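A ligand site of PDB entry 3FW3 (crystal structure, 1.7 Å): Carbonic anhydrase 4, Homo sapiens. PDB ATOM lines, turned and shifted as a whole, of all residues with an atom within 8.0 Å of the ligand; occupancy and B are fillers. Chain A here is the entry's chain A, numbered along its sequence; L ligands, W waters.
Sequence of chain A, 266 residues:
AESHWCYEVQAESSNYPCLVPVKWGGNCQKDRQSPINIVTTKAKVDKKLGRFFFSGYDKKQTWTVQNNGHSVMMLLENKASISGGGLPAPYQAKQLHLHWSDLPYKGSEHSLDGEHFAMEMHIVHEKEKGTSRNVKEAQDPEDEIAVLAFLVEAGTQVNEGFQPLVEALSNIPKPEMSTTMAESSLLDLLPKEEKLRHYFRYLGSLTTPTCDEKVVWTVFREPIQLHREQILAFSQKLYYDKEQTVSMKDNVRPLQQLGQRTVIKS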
ATOM      1  N   GLU A 153       9.816  29.116 -20.264  1.00  0.00           N
ATOM      2  CA  GLU A 153       8.443  29.322 -19.762  1.00  0.00           C
ATOM      3  C   GLU A 153       7.498  28.224 -20.241  1.00  0.00           C
ATOM      4  O   GLU A 153       7.812  27.466 -21.156  1.00  0.00           O
ATOM      5  CB  GLU A 153       7.898  30.697 -20.178  1.00  0.00           C
ATOM      6  CG  GLU A 153       7.658  30.882 -21.677  1.00  0.00           C
ATOM      7  CD  GLU A 153       7.417  32.342 -22.089  1.00  0.00           C
ATOM      8  OE1 GLU A 153       7.596  33.298 -21.300  1.00  0.00           O
ATOM      9  OE2 GLU A 153       7.057  32.532 -23.244  1.00  0.00           O
ATOM     10  N   ALA A 154       6.336  28.142 -19.599  1.00  0.00           N
ATOM     11  CA  ALA A 154       5.294  27.206 -20.045  1.00  0.00           C
ATOM     12  C   ALA A 154       4.635  27.697 -21.337  1.00  0.00           C
ATOM     13  O   ALA A 154       4.272  28.872 -21.445  1.00  0.00           O
ATOM     14  CB  ALA A 154       4.240  27.015 -18.932  1.00  0.00           C
ATOM     15  N   GLY A 155       4.537  26.815 -22.327  1.00  0.00           N
ATOM     16  CA  GLY A 155       3.796  27.085 -23.552  1.00  0.00           C
ATOM     17  C   GLY A 155       2.608  26.146 -23.707  1.00  0.00           C
ATOM     18  O   GLY A 155       2.236  25.428 -22.768  1.00  0.00           O
ATOM     19  N   THR A 156       2.082  26.109 -24.914  1.00  0.00           N
ATOM     20  CA  THR A 156       0.865  25.352 -25.224  1.00  0.00           C
ATOM     21  C   THR A 156       1.100  23.856 -25.490  1.00  0.00           C
ATOM     22  O   THR A 156       0.162  23.081 -25.482  1.00  0.00           O
ATOM     23  CB  THR A 156       0.148  25.960 -26.468  1.00  0.00           C
ATOM     24  OG1 THR A 156       1.038  25.998 -27.572  1.00  0.00           O
ATOM     25  CG2 THR A 156      -0.205  27.441 -26.242  1.00  0.00           C
ATOM     26  N   GLN A 157       2.346  23.481 -25.769  1.00  0.00           N
ATOM     27  CA  GLN A 157       2.646  22.170 -26.336  1.00  0.00           C
ATOM     28  C   GLN A 157       3.852  21.517 -25.688  1.00  0.00           C
ATOM     29  O   GLN A 157       4.707  22.200 -25.126  1.00  0.00           O
ATOM     30  CB  GLN A 157       2.911  22.302 -27.827  1.00  0.00           C
ATOM     31  CG  GLN A 157       1.697  22.699 -28.650  1.00  0.00           C
ATOM     32  CD  GLN A 157       2.060  23.122 -30.040  1.00  0.00           C
ATOM     33  OE1 GLN A 157       2.343  22.288 -30.897  1.00  0.00           O
ATOM     34  NE2 GLN A 157       2.088  24.421 -30.279  1.00  0.00           N
ATOM     35  N   VAL A 158       3.911  20.183 -25.822  1.00  0.00           N
ATOM     36  CA  VAL A 158       5.133  19.433 -25.494  1.00  0.00           C
ATOM     37  C   VAL A 158       6.269  19.855 -26.450  1.00  0.00           C
ATOM     38  O   VAL A 158       6.137  19.864 -27.692  1.00  0.00           O
ATOM     39  CB  VAL A 158       4.904  17.919 -25.625  1.00  0.00           C
ATOM     40  CG1 VAL A 158       6.231  17.163 -25.459  1.00  0.00           C
ATOM     41  CG2 VAL A 158       3.874  17.480 -24.618  1.00  0.00           C
ATOM     42  N   ASN A 159       7.417  20.158 -25.866  1.00  0.00           N
ATOM     43  CA  ASN A 159       8.603  20.467 -26.617  1.00  0.00           C
ATOM     44  C   ASN A 159       9.276  19.120 -26.848  1.00  0.00           C
ATOM     45  O   ASN A 159       9.885  18.554 -25.949  1.00  0.00           O
ATOM     46  CB  ASN A 159       9.482  21.459 -25.836  1.00  0.00           C
ATOM     47  CG  ASN A 159      10.695  21.901 -26.604  1.00  0.00           C
ATOM     48  OD1 ASN A 159      11.246  21.110 -27.357  1.00  0.00           O
ATOM     49  ND2 ASN A 159      11.113  23.166 -26.457  1.00  0.00           N
ATOM     50  N   GLU A 160       9.145  18.606 -28.067  1.00  0.00           N
ATOM     51  CA  GLU A 160       9.617  17.277 -28.373  1.00  0.00           C
ATOM     52  C   GLU A 160      11.115  17.144 -28.227  1.00  0.00           C
ATOM     53  O   GLU A 160      11.613  16.058 -27.858  1.00  0.00           O
ATOM     54  CB  GLU A 160       9.213  16.885 -29.796  1.00  0.00           C
ATOM     55  CG  GLU A 160       7.709  16.776 -30.002  1.00  0.00           C
ATOM     56  CD  GLU A 160       7.038  15.684 -29.171  1.00  0.00           C
ATOM     57  OE1 GLU A 160       7.675  14.655 -28.846  1.00  0.00           O
ATOM     58  OE2 GLU A 160       5.845  15.885 -28.849  1.00  0.00           O
ATOM     59  N   GLY A 161      11.834  18.219 -28.537  1.00  0.00           N
ATOM     60  CA  GLY A 161      13.270  18.237 -28.382  1.00  0.00           C
ATOM     61  C   GLY A 161      13.793  17.962 -26.981  1.00  0.00           C
ATOM     62  O   GLY A 161      14.894  17.396 -26.816  1.00  0.00           O
ATOM     63  N   PHE A 162      13.010  18.373 -25.986  1.00  0.00           N
ATOM     64  CA  PHE A 162      13.306  18.105 -24.573  1.00  0.00           C
ATOM     65  C   PHE A 162      12.892  16.718 -24.061  1.00  0.00           C
ATOM     66  O   PHE A 162      13.274  16.352 -22.937  1.00  0.00           O
ATOM     67  CB  PHE A 162      12.687  19.171 -23.652  1.00  0.00           C
ATOM     68  CG  PHE A 162      13.530  20.401 -23.520  1.00  0.00           C
ATOM     69  CD1 PHE A 162      13.636  21.298 -24.561  1.00  0.00           C
ATOM     70  CD2 PHE A 162      14.201  20.698 -22.312  1.00  0.00           C
ATOM     71  CE1 PHE A 162      14.430  22.443 -24.444  1.00  0.00           C
ATOM     72  CE2 PHE A 162      14.965  21.874 -22.181  1.00  0.00           C
ATOM     73  CZ  PHE A 162      15.084  22.726 -23.265  1.00  0.00           C
ATOM     74  N   ASP A 188      17.998  20.442 -30.911  1.00  0.00           N
ATOM     75  CA  ASP A 188      16.632  20.067 -30.493  1.00  0.00           C
ATOM     76  C   ASP A 188      16.168  20.847 -29.238  1.00  0.00           C
ATOM     77  O   ASP A 188      14.937  20.932 -28.986  1.00  0.00           O
ATOM     78  CB  ASP A 188      16.560  18.580 -30.074  1.00  0.00           C
ATOM     79  CG  ASP A 188      16.631  17.582 -31.233  1.00  0.00           C
ATOM     80  OD1 ASP A 188      16.318  17.954 -32.399  1.00  0.00           O
ATOM     81  OD2 ASP A 188      16.950  16.358 -30.997  1.00  0.00           O
ATOM     82  N   LEU A 190      17.175  24.077 -28.494  1.00  0.00           N
ATOM     83  CA  LEU A 190      17.238  25.538 -28.683  1.00  0.00           C
ATOM     84  C   LEU A 190      16.099  26.108 -29.518  1.00  0.00           C
ATOM     85  O   LEU A 190      15.492  25.394 -30.323  1.00  0.00           O
ATOM     86  CB  LEU A 190      18.533  25.905 -29.388  1.00  0.00           C
ATOM     87  CG  LEU A 190      19.850  25.502 -28.726  1.00  0.00           C
ATOM     88  CD1 LEU A 190      20.993  26.220 -29.424  1.00  0.00           C
ATOM     89  CD2 LEU A 190      19.833  25.737 -27.239  1.00  0.00           C
ATOM     90  N   ILE A 224      12.559  29.788 -24.437  1.00  0.00           N
ATOM     91  CA  ILE A 224      12.144  28.420 -24.827  1.00  0.00           C
ATOM     92  C   ILE A 224      10.824  28.131 -24.149  1.00  0.00           C
ATOM     93  O   ILE A 224      10.619  28.526 -23.001  1.00  0.00           O
ATOM     94  CB  ILE A 224      13.151  27.420 -24.308  1.00  0.00           C
ATOM     95  CG1 ILE A 224      14.480  27.535 -25.014  1.00  0.00           C
ATOM     96  CG2 ILE A 224      12.678  25.968 -24.516  1.00  0.00           C
ATOM     97  CD1 ILE A 224      15.560  26.724 -24.355  1.00  0.00           C
ATOM     98  N   GLN A 225       9.954  27.387 -24.817  1.00  0.00           N
ATOM     99  CA  GLN A 225       8.692  26.960 -24.228  1.00  0.00           C
ATOM    100  C   GLN A 225       8.654  25.448 -24.044  1.00  0.00           C
ATOM    101  O   GLN A 225       8.916  24.698 -24.985  1.00  0.00           O
ATOM    102  CB  GLN A 225       7.534  27.415 -25.122  1.00  0.00           C
ATOM    103  CG  GLN A 225       7.449  28.983 -25.191  1.00  0.00           C
ATOM    104  CD  GLN A 225       6.156  29.488 -25.892  1.00  0.00           C
ATOM    105  OE1 GLN A 225       5.820  29.011 -26.967  1.00  0.00           O
ATOM    106  NE2 GLN A 225       5.493  30.460 -25.292  1.00  0.00           N
ATOM    107  N   LEU A 226       8.331  25.021 -22.831  1.00  0.00           N
ATOM    108  CA  LEU A 226       8.054  23.618 -22.534  1.00  0.00           C
ATOM    109  C   LEU A 226       6.583  23.529 -22.088  1.00  0.00           C
ATOM    110  O   LEU A 226       6.045  24.508 -21.590  1.00  0.00           O
ATOM    111  CB  LEU A 226       8.963  23.159 -21.375  1.00  0.00           C
ATOM    112  CG  LEU A 226      10.295  22.486 -21.740  1.00  0.00           C
ATOM    113  CD1 LEU A 226      11.153  23.389 -22.528  1.00  0.00           C
ATOM    114  CD2 LEU A 226      11.018  21.922 -20.508  1.00  0.00           C
ATOM    115  N   HIS A 227       5.962  22.368 -22.219  1.00  0.00           N
ATOM    116  CA  HIS A 227       4.652  22.144 -21.591  1.00  0.00           C
ATOM    117  C   HIS A 227       4.791  22.183 -20.063  1.00  0.00           C
ATOM    118  O   HIS A 227       5.834  21.796 -19.495  1.00  0.00           O
ATOM    119  CB  HIS A 227       4.056  20.787 -22.039  1.00  0.00           C
ATOM    120  CG  HIS A 227       2.605  20.606 -21.697  1.00  0.00           C
ATOM    121  ND1 HIS A 227       2.161  20.405 -20.399  1.00  0.00           N
ATOM    122  CD2 HIS A 227       1.509  20.497 -22.487  1.00  0.00           C
ATOM    123  CE1 HIS A 227       0.845  20.243 -20.407  1.00  0.00           C
ATOM    124  NE2 HIS A 227       0.425  20.301 -21.650  1.00  0.00           N
ATOM    125  N   GLN A 230       6.195  19.031 -18.496  1.00  0.00           N
ATOM    126  CA  GLN A 230       7.639  18.800 -18.703  1.00  0.00           C
ATOM    127  C   GLN A 230       8.449  19.585 -17.678  1.00  0.00           C
ATOM    128  O   GLN A 230       9.428  19.098 -17.124  1.00  0.00           O
ATOM    129  CB  GLN A 230       8.076  19.198 -20.110  1.00  0.00           C
ATOM    130  CG  GLN A 230       7.540  18.338 -21.263  1.00  0.00           C
ATOM    131  CD  GLN A 230       8.018  18.867 -22.595  1.00  0.00           C
ATOM    132  OE1 GLN A 230       7.648  19.993 -22.990  1.00  0.00           O
ATOM    133  NE2 GLN A 230       8.945  18.117 -23.255  1.00  0.00           N
HETATM  134  C1  LIG L   1       7.293  24.077 -27.759  1.00  0.00           C
HETATM  135  C2  LIG L   1       7.309  23.298 -29.087  1.00  0.00           C
HETATM  136  C3  LIG L   1       7.056  24.297 -30.224  1.00  0.00           C
HETATM  137  C4  LIG L   1       5.721  24.990 -30.011  1.00  0.00           C
HETATM  138  C5  LIG L   1       5.668  25.604 -28.623  1.00  0.00           C
HETATM  139  C6  LIG L   1       4.297  26.213 -28.363  1.00  0.00           C
HETATM  140  O1  LIG L   1       8.561  22.684 -29.229  1.00  0.00           O
HETATM  141  O2  LIG L   1       7.045  23.712 -31.495  1.00  0.00           O
HETATM  142  O3  LIG L   1       5.607  25.990 -31.017  1.00  0.00           O
HETATM  143  O4  LIG L   1       5.955  24.606 -27.656  1.00  0.00           O
HETATM  144  O5  LIG L   1       4.356  26.895 -27.126  1.00  0.00           O
HETATM  145  O   HOH W   1       9.563  23.443 -32.703  1.00  0.00           O
HETATM  146  O   HOH W   2       5.156  24.773 -24.770  1.00  0.00           O
HETATM  147  O   HOH W   3       8.363  20.221 -30.400  1.00  0.00           O
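Water W3 lies within hydrogen-bond range of an oxygen (O1) of the ligand (2.7 Å) and the backbone NH of Glu 160 (2.9 Å).
An oxygen (O5) of the ligand sits at hydrogen-bond distance from the side-chain amide oxygen (OE1) of Gln 225.
The backbone NH (N) of Thr 156 sits at hydrogen-bond distance from an oxygen (O5) of the ligand (3.3 Å).
The side-chain hydroxyl (OG1) of Thr 156 lies close to an oxygen (O5) of the ligand (3.5 Å).
The backbone carbonyl oxygen (O) of Gln 225 sits at hydrogen-bond distance from the side-chain amide nitrogen (ND2) of Asn 159 (3.1 Å).
NE2 of Gln 225 lies within hydrogen-bond range of OE2 of Glu 153 (3.3 Å).
OG1 of Thr 156 is in hydrogen-bond range of NE2 of Gln 157 (3.3 Å).
N of Gly 161 lies within hydrogen-bond range of OD1 of Asn 159, at 3.2 Å.
The backbone carbonyl oxygen of Asn 159 lies within hydrogen-bond range of the side-chain amide nitrogen of Gln 230 (2.9 Å).
The backbone carbonyl oxygen (O) of Gln 157 lies within hydrogen-bond range of the backbone NH (N) of His 227 (3.2 Å).
The backbone NH (N) of Gly 155 lies within hydrogen-bond range of the backbone carbonyl oxygen (O) of Leu 226 (2.9 Å).
Residues that only touch the ligand: Asn 159 (3.4 Å), Gln 157 (3.4 Å), Gly 155 (3.6 Å) and Val 158 (3.9 Å).
Of the 17 residues printed, 6 come within 4 Å of the ligand.
The nearest printed residue that does not touch the ligand is Glu 160 (4.3 Å).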
